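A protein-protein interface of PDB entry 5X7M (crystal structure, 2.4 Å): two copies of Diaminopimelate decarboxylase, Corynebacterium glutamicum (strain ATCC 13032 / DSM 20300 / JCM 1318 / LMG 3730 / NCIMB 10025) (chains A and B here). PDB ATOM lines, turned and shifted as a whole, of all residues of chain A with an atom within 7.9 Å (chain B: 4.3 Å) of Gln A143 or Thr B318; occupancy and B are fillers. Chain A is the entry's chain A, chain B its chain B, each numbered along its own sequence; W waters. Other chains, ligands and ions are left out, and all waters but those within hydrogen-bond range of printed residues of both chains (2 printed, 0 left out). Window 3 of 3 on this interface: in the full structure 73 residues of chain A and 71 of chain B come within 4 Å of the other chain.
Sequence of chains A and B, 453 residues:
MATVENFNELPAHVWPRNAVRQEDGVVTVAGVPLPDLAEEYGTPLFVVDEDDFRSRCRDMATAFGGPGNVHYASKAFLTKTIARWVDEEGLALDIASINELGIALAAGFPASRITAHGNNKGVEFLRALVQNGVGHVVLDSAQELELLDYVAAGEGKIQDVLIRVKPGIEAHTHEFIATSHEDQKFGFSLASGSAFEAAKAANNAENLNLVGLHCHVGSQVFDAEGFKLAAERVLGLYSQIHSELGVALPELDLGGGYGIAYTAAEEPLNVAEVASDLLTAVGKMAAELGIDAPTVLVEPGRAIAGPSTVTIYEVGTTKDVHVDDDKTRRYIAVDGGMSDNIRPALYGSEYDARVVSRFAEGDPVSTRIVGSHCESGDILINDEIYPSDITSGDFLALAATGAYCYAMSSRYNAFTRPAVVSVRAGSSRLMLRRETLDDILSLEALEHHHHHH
ND2 of Asn A120 sits close to N of Thr B317 (3.0 Å). OE1 of Gln A143 lies close to O of Thr B318, at 3.0 Å. The side-chain carboxylate (OD2) of Asp A140 lies within salt-bridge range of the side-chain amino group (NZ) of Lys B319, at 3.2 Å.
The side-chain carboxylate of Glu A144 lies within hydrogen-bond range of the backbone NH of Asp A140. The side-chain hydroxyl (OG) of Ser A141 sits at hydrogen-bond distance from the backbone NH (N) of Glu A144, at 3.0 Å. The backbone NH (N) of Gln A143 sits close to the side-chain hydroxyl (OG) of Ser A141 (3.5 Å). The backbone carbonyl oxygen (O) of Lys B319 is in hydrogen-bond range of the backbone NH (N) of Tyr B331, at 2.9 Å.
Thr B317 touches Asn A119 (OG1 to O, 3.6 Å). ND2 of Asn A120 touches CA of Gly B316, 3.4 Å away. Ser A141 touches Thr B317. Gln A143 touches Thr B317 (NE2 to CA, 3.5 Å).
Of the printed residues of chain B, Asn A119 touches Thr B317 (3.6 Å). Of the printed residues of chain B, Asp A140 touches Lys B319. Of the printed residues of chain B, Ser A141 touches Thr B317 (3.7 Å). Of the printed residues of chain B, Gln A143 touches Thr B317 and Thr B318. Val B315 touches none of the printed residues of chain A. Printed residues of chain A within 4 Å of Gly B316: Asn A120. Of the printed residues of chain A, Thr B317 touches Asn A119, Asn A120, Ser A141 and Gln A143. Thr B318 touches just one residue of chain A: Gln A143. Ile B390 touches none of the printed residues of chain A. The nearest printed residue of chain B that does not touch Gln A143 is Gly B316 (4.02 Å).
Printed residues of chain B that touch a printed residue of chain A: Gly B316, Thr B317, Thr B318 and Lys B319. Among the printed residues, 7 pairs touch across the chains. Among the printed residues, Asp or Glu carboxylates within 4 Å of a Lys or Arg side-chain nitrogen of the other chain: Asp A140 with Lys B319 (3.2 Å).
No position is printed for both chains.
Water W1 bridges OE1 of Gln A143 (3.2 Å) and O of Thr B318 (3.3 Å). Water W2 bridges the side-chain amide oxygen (OD1) of Asn A120 (3.2 Å) and the backbone NH (N) of Gly B316 (3.4 Å).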
ATOM      1  N   ASN A 119       2.451  17.639  -4.784  1.00  0.00           N
ATOM      2  CA  ASN A 119       3.702  17.567  -4.010  1.00  0.00           C
ATOM      3  C   ASN A 119       4.882  17.044  -4.782  1.00  0.00           C
ATOM      4  O   ASN A 119       5.971  16.985  -4.235  1.00  0.00           O
ATOM      5  CB  ASN A 119       3.543  16.661  -2.800  1.00  0.00           C
ATOM      6  CG  ASN A 119       3.518  15.206  -3.187  1.00  0.00           C
ATOM      7  OD1 ASN A 119       2.599  14.788  -3.876  1.00  0.00           O
ATOM      8  ND2 ASN A 119       4.571  14.455  -2.832  1.00  0.00           N
ATOM      9  N   ASN A 120       4.665  16.619  -6.017  1.00  0.00           N
ATOM     10  CA  ASN A 120       5.730  16.123  -6.864  1.00  0.00           C
ATOM     11  C   ASN A 120       5.395  16.403  -8.359  1.00  0.00           C
ATOM     12  O   ASN A 120       5.241  15.500  -9.197  1.00  0.00           O
ATOM     13  CB  ASN A 120       5.873  14.625  -6.578  1.00  0.00           C
ATOM     14  CG  ASN A 120       7.007  13.972  -7.344  1.00  0.00           C
ATOM     15  OD1 ASN A 120       6.899  12.800  -7.760  1.00  0.00           O
ATOM     16  ND2 ASN A 120       8.075  14.732  -7.572  1.00  0.00           N
ATOM     17  N   LYS A 121       5.209  17.672  -8.648  1.00  0.00           N
ATOM     18  CA  LYS A 121       4.913  18.107  -9.995  1.00  0.00           C
ATOM     19  C   LYS A 121       6.108  17.866 -10.918  1.00  0.00           C
ATOM     20  O   LYS A 121       7.181  18.465 -10.730  1.00  0.00           O
ATOM     21  CB  LYS A 121       4.568  19.603 -10.012  1.00  0.00           C
ATOM     22  CG  LYS A 121       3.242  19.913  -9.361  1.00  0.00           C
ATOM     23  CD  LYS A 121       2.861  21.389  -9.520  1.00  0.00           C
ATOM     24  CE  LYS A 121       1.902  21.840  -8.442  1.00  0.00           C
ATOM     25  NZ  LYS A 121       2.541  21.912  -7.089  1.00  0.00           N
ATOM     26  N   LEU A 126       4.349  20.980 -15.052  1.00  0.00           N
ATOM     27  CA  LEU A 126       4.643  22.387 -14.927  1.00  0.00           C
ATOM     28  C   LEU A 126       4.534  23.146 -16.249  1.00  0.00           C
ATOM     29  O   LEU A 126       4.011  24.242 -16.298  1.00  0.00           O
ATOM     30  CB  LEU A 126       6.039  22.561 -14.343  1.00  0.00           C
ATOM     31  CG  LEU A 126       6.142  22.056 -12.899  1.00  0.00           C
ATOM     32  CD1 LEU A 126       7.592  22.154 -12.447  1.00  0.00           C
ATOM     33  CD2 LEU A 126       5.196  22.831 -11.995  1.00  0.00           C
ATOM     34  N   LEU A 139       3.393  26.063  -4.748  1.00  0.00           N
ATOM     35  CA  LEU A 139       4.729  25.500  -4.695  1.00  0.00           C
ATOM     36  C   LEU A 139       4.833  24.654  -3.438  1.00  0.00           C
ATOM     37  O   LEU A 139       4.436  25.114  -2.366  1.00  0.00           O
ATOM     38  CB  LEU A 139       5.792  26.615  -4.703  1.00  0.00           C
ATOM     39  CG  LEU A 139       5.829  27.509  -5.946  1.00  0.00           C
ATOM     40  CD1 LEU A 139       6.830  28.660  -5.775  1.00  0.00           C
ATOM     41  CD2 LEU A 139       6.146  26.706  -7.201  1.00  0.00           C
ATOM     42  N   ASP A 140       5.368  23.430  -3.590  1.00  0.00           N
ATOM     43  CA  ASP A 140       5.481  22.449  -2.522  1.00  0.00           C
ATOM     44  C   ASP A 140       6.914  22.173  -1.988  1.00  0.00           C
ATOM     45  O   ASP A 140       7.077  21.750  -0.828  1.00  0.00           O
ATOM     46  CB  ASP A 140       4.855  21.134  -2.971  1.00  0.00           C
ATOM     47  CG  ASP A 140       4.583  20.214  -1.784  1.00  0.00           C
ATOM     48  OD1 ASP A 140       3.569  20.449  -1.064  1.00  0.00           O
ATOM     49  OD2 ASP A 140       5.433  19.328  -1.536  1.00  0.00           O
ATOM     50  N   SER A 141       7.947  22.425  -2.807  1.00  0.00           N
ATOM     51  CA  SER A 141       9.340  22.202  -2.414  1.00  0.00           C
ATOM     52  C   SER A 141      10.235  23.227  -3.030  1.00  0.00           C
ATOM     53  O   SER A 141       9.922  23.813  -4.095  1.00  0.00           O
ATOM     54  CB  SER A 141       9.798  20.869  -2.976  1.00  0.00           C
ATOM     55  OG  SER A 141       9.630  20.862  -4.388  1.00  0.00           O
ATOM     56  N   ALA A 142      11.393  23.396  -2.402  1.00  0.00           N
ATOM     57  CA  ALA A 142      12.493  24.144  -2.999  1.00  0.00           C
ATOM     58  C   ALA A 142      12.778  23.753  -4.477  1.00  0.00           C
ATOM     59  O   ALA A 142      13.038  24.631  -5.289  1.00  0.00           O
ATOM     60  CB  ALA A 142      13.741  23.995  -2.148  1.00  0.00           C
ATOM     61  N   GLN A 143      12.679  22.461  -4.812  1.00  0.00           N
ATOM     62  CA  GLN A 143      12.926  21.958  -6.173  1.00  0.00           C
ATOM     63  C   GLN A 143      11.850  22.337  -7.166  1.00  0.00           C
ATOM     64  O   GLN A 143      12.110  22.541  -8.333  1.00  0.00           O
ATOM     65  CB  GLN A 143      13.069  20.428  -6.183  1.00  0.00           C
ATOM     66  CG  GLN A 143      14.298  19.943  -5.420  1.00  0.00           C
ATOM     67  CD  GLN A 143      14.251  18.475  -4.984  1.00  0.00           C
ATOM     68  OE1 GLN A 143      14.868  18.080  -3.972  1.00  0.00           O
ATOM     69  NE2 GLN A 143      13.577  17.658  -5.769  1.00  0.00           N
ATOM     70  N   GLU A 144      10.617  22.375  -6.747  1.00  0.00           N
ATOM     71  CA  GLU A 144       9.592  22.762  -7.690  1.00  0.00           C
ATOM     72  C   GLU A 144       9.737  24.261  -8.001  1.00  0.00           C
ATOM     73  O   GLU A 144       9.512  24.672  -9.116  1.00  0.00           O
ATOM     74  CB  GLU A 144       8.228  22.439  -7.121  1.00  0.00           C
ATOM     75  CG  GLU A 144       7.081  23.005  -7.904  1.00  0.00           C
ATOM     76  CD  GLU A 144       5.785  22.819  -7.168  1.00  0.00           C
ATOM     77  OE1 GLU A 144       5.806  22.273  -6.029  1.00  0.00           O
ATOM     78  OE2 GLU A 144       4.734  23.206  -7.750  1.00  0.00           O
ATOM     79  N   LEU A 145      10.099  25.051  -6.996  1.00  0.00           N
ATOM     80  CA  LEU A 145      10.305  26.475  -7.149  1.00  0.00           C
ATOM     81  C   LEU A 145      11.365  26.718  -8.210  1.00  0.00           C
ATOM     82  O   LEU A 145      11.075  27.353  -9.240  1.00  0.00           O
ATOM     83  CB  LEU A 145      10.701  27.112  -5.818  1.00  0.00           C
ATOM     84  CG  LEU A 145      10.716  28.639  -5.769  1.00  0.00           C
ATOM     85  CD1 LEU A 145      10.364  29.112  -4.357  1.00  0.00           C
ATOM     86  CD2 LEU A 145      12.069  29.223  -6.201  1.00  0.00           C
ATOM     87  N   GLU A 146      12.568  26.182  -8.012  1.00  0.00           N
ATOM     88  CA  GLU A 146      13.634  26.422  -9.010  1.00  0.00           C
ATOM     89  C   GLU A 146      13.250  25.928 -10.391  1.00  0.00           C
ATOM     90  O   GLU A 146      13.487  26.629 -11.380  1.00  0.00           O
ATOM     91  CB  GLU A 146      15.014  25.942  -8.570  1.00  0.00           C
ATOM     92  CG  GLU A 146      15.196  24.465  -8.271  1.00  0.00           C
ATOM     93  CD  GLU A 146      16.267  24.162  -7.194  1.00  0.00           C
ATOM     94  OE1 GLU A 146      17.023  25.082  -6.772  1.00  0.00           O
ATOM     95  OE2 GLU A 146      16.340  22.981  -6.752  1.00  0.00           O
ATOM     96  N   LEU A 147      12.567  24.792 -10.446  1.00  0.00           N
ATOM     97  CA  LEU A 147      12.169  24.188 -11.720  1.00  0.00           C
ATOM     98  C   LEU A 147      11.052  24.964 -12.383  1.00  0.00           C
ATOM     99  O   LEU A 147      11.016  25.043 -13.598  1.00  0.00           O
ATOM    100  CB  LEU A 147      11.749  22.731 -11.519  1.00  0.00           C
ATOM    101  CG  LEU A 147      11.301  21.939 -12.755  1.00  0.00           C
ATOM    102  CD1 LEU A 147      12.430  21.814 -13.775  1.00  0.00           C
ATOM    103  CD2 LEU A 147      10.785  20.560 -12.335  1.00  0.00           C
ATOM    104  N   LEU A 148      10.126  25.515 -11.603  1.00  0.00           N
ATOM    105  CA  LEU A 148       9.041  26.314 -12.162  1.00  0.00           C
ATOM    106  C   LEU A 148       9.593  27.644 -12.682  1.00  0.00           C
ATOM    107  O   LEU A 148       9.085  28.213 -13.628  1.00  0.00           O
ATOM    108  CB  LEU A 148       7.931  26.576 -11.127  1.00  0.00           C
ATOM    109  CG  LEU A 148       6.705  27.353 -11.670  1.00  0.00           C
ATOM    110  CD1 LEU A 148       6.105  26.688 -12.903  1.00  0.00           C
ATOM    111  CD2 LEU A 148       5.642  27.564 -10.602  1.00  0.00           C
ATOM    112  N   ASP A 149      10.623  28.148 -12.036  1.00  0.00           N
ATOM    113  CA  ASP A 149      11.272  29.352 -12.506  1.00  0.00           C
ATOM    114  C   ASP A 149      11.883  29.111 -13.901  1.00  0.00           C
ATOM    115  O   ASP A 149      11.603  29.875 -14.832  1.00  0.00           O
ATOM    116  CB  ASP A 149      12.318  29.812 -11.488  1.00  0.00           C
ATOM    117  CG  ASP A 149      12.807  31.243 -11.737  1.00  0.00           C
ATOM    118  OD1 ASP A 149      12.048  32.061 -12.329  1.00  0.00           O
ATOM    119  OD2 ASP A 149      13.949  31.543 -11.307  1.00  0.00           O
ATOM    120  N   PHE A 188       6.283  23.723   3.294  1.00  0.00           N
ATOM    121  CA  PHE A 188       7.443  24.186   4.042  1.00  0.00           C
ATOM    122  C   PHE A 188       7.024  24.423   5.499  1.00  0.00           C
ATOM    123  O   PHE A 188       5.950  24.997   5.687  1.00  0.00           O
ATOM    124  CB  PHE A 188       7.923  25.505   3.419  1.00  0.00           C
ATOM    125  CG  PHE A 188       8.336  25.422   1.945  1.00  0.00           C
ATOM    126  CD1 PHE A 188       7.394  25.524   0.932  1.00  0.00           C
ATOM    127  CD2 PHE A 188       9.690  25.310   1.577  1.00  0.00           C
ATOM    128  CE1 PHE A 188       7.764  25.489  -0.390  1.00  0.00           C
ATOM    129  CE2 PHE A 188      10.059  25.265   0.233  1.00  0.00           C
ATOM    130  CZ  PHE A 188       9.092  25.373  -0.739  1.00  0.00           C
ATOM    131  N   VAL B 315      11.995   8.397  -8.889  1.00  0.00           N
ATOM    132  CA  VAL B 315      12.061   9.311  -7.764  1.00  0.00           C
ATOM    133  C   VAL B 315      11.938  10.726  -8.289  1.00  0.00           C
ATOM    134  O   VAL B 315      12.582  11.059  -9.264  1.00  0.00           O
ATOM    135  CB  VAL B 315      13.388   9.114  -7.026  1.00  0.00           C
ATOM    136  CG1 VAL B 315      13.617  10.213  -6.017  1.00  0.00           C
ATOM    137  CG2 VAL B 315      13.373   7.742  -6.397  1.00  0.00           C
ATOM    138  N   GLY B 316      11.081  11.529  -7.655  1.00  0.00           N
ATOM    139  CA  GLY B 316      10.938  12.946  -7.931  1.00  0.00           C
ATOM    140  C   GLY B 316      11.479  13.773  -6.766  1.00  0.00           C
ATOM    141  O   GLY B 316      12.689  13.809  -6.510  1.00  0.00           O
ATOM    142  N   THR B 317      10.582  14.374  -6.000  1.00  0.00           N
ATOM    143  CA  THR B 317      10.960  15.392  -5.033  1.00  0.00           C
ATOM    144  C   THR B 317      11.624  14.745  -3.840  1.00  0.00           C
ATOM    145  O   THR B 317      11.256  13.671  -3.473  1.00  0.00           O
ATOM    146  CB  THR B 317       9.736  16.215  -4.612  1.00  0.00           C
ATOM    147  OG1 THR B 317       9.197  16.894  -5.759  1.00  0.00           O
ATOM    148  CG2 THR B 317      10.089  17.247  -3.595  1.00  0.00           C
ATOM    149  N   THR B 318      12.629  15.371  -3.248  1.00  0.00           N
ATOM    150  CA  THR B 318      13.124  14.878  -1.963  1.00  0.00           C
ATOM    151  C   THR B 318      13.266  16.038  -1.001  1.00  0.00           C
ATOM    152  O   THR B 318      13.647  17.130  -1.391  1.00  0.00           O
ATOM    153  CB  THR B 318      14.476  14.155  -2.118  1.00  0.00           C
ATOM    154  OG1 THR B 318      15.483  15.109  -2.452  1.00  0.00           O
ATOM    155  CG2 THR B 318      14.421  13.084  -3.233  1.00  0.00           C
ATOM    156  N   LYS B 319      12.964  15.824   0.262  1.00  0.00           N
ATOM    157  CA  LYS B 319      13.199  16.868   1.229  1.00  0.00           C
ATOM    158  C   LYS B 319      13.343  16.384   2.632  1.00  0.00           C
ATOM    159  O   LYS B 319      12.825  15.345   2.993  1.00  0.00           O
ATOM    160  CB  LYS B 319      12.047  17.872   1.199  1.00  0.00           C
ATOM    161  CG  LYS B 319      10.697  17.292   1.572  1.00  0.00           C
ATOM    162  CD  LYS B 319       9.567  17.893   0.733  1.00  0.00           C
ATOM    163  CE  LYS B 319       8.937  19.092   1.375  1.00  0.00           C
ATOM    164  NZ  LYS B 319       7.538  19.210   0.895  1.00  0.00           N
ATOM    165  N   ARG B 330      13.610  12.186   6.038  1.00  0.00           N
ATOM    166  CA  ARG B 330      13.759  12.385   4.611  1.00  0.00           C
ATOM    167  C   ARG B 330      12.520  11.845   3.910  1.00  0.00           C
ATOM    168  O   ARG B 330      12.165  10.711   4.117  1.00  0.00           O
ATOM    169  CB  ARG B 330      15.062  11.745   4.091  1.00  0.00           C
ATOM    170  CG  ARG B 330      15.616  12.412   2.823  1.00  0.00           C
ATOM    171  CD  ARG B 330      17.126  12.296   2.670  1.00  0.00           C
ATOM    172  NE  ARG B 330      17.513  12.675   1.311  1.00  0.00           N
ATOM    173  CZ  ARG B 330      17.429  11.909   0.208  1.00  0.00           C
ATOM    174  NH1 ARG B 330      17.008  10.649   0.238  1.00  0.00           N
ATOM    175  NH2 ARG B 330      17.791  12.416  -0.959  1.00  0.00           N
ATOM    176  N   TYR B 331      11.847  12.669   3.115  1.00  0.00           N
ATOM    177  CA  TYR B 331      10.675  12.250   2.359  1.00  0.00           C
ATOM    178  C   TYR B 331      11.083  12.110   0.897  1.00  0.00           C
ATOM    179  O   TYR B 331      11.621  13.043   0.297  1.00  0.00           O
ATOM    180  CB  TYR B 331       9.568  13.293   2.472  1.00  0.00           C
ATOM    181  CG  TYR B 331       8.691  13.141   3.675  1.00  0.00           C
ATOM    182  CD1 TYR B 331       9.177  13.414   4.956  1.00  0.00           C
ATOM    183  CD2 TYR B 331       7.361  12.708   3.558  1.00  0.00           C
ATOM    184  CE1 TYR B 331       8.374  13.246   6.075  1.00  0.00           C
ATOM    185  CE2 TYR B 331       6.553  12.553   4.686  1.00  0.00           C
ATOM    186  CZ  TYR B 331       7.069  12.835   5.929  1.00  0.00           C
ATOM    187  OH  TYR B 331       6.299  12.692   7.043  1.00  0.00           O
ATOM    188  N   ILE B 332      10.829  10.958   0.312  1.00  0.00           N
ATOM    189  CA  ILE B 332      11.125  10.740  -1.102  1.00  0.00           C
ATOM    190  C   ILE B 332       9.801  10.569  -1.769  1.00  0.00           C
ATOM    191  O   ILE B 332       9.036   9.687  -1.430  1.00  0.00           O
ATOM    192  CB  ILE B 332      12.015   9.484  -1.355  1.00  0.00           C
ATOM    193  CG1 ILE B 332      13.297   9.555  -0.535  1.00  0.00           C
ATOM    194  CG2 ILE B 332      12.404   9.352  -2.823  1.00  0.00           C
ATOM    195  CD1 ILE B 332      14.037   8.250  -0.482  1.00  0.00           C
ATOM    196  N   ILE B 390      19.728   8.952  -2.231  1.00  0.00           N
ATOM    197  CA  ILE B 390      18.662   8.607  -3.180  1.00  0.00           C
ATOM    198  C   ILE B 390      18.111   9.923  -3.690  1.00  0.00           C
ATOM    199  O   ILE B 390      17.899  10.842  -2.919  1.00  0.00           O
ATOM    200  CB  ILE B 390      17.544   7.793  -2.549  1.00  0.00           C
ATOM    201  CG1 ILE B 390      18.076   6.401  -2.182  1.00  0.00           C
ATOM    202  CG2 ILE B 390      16.358   7.712  -3.528  1.00  0.00           C
ATOM    203  CD1 ILE B 390      17.274   5.685  -1.121  1.00  0.00           C
HETATM  204  O   HOH W   1      13.168  20.228  -2.406  1.00  0.00           O
HETATM  205  O   HOH W   2       8.666  11.555 -10.077  1.00  0.00           O
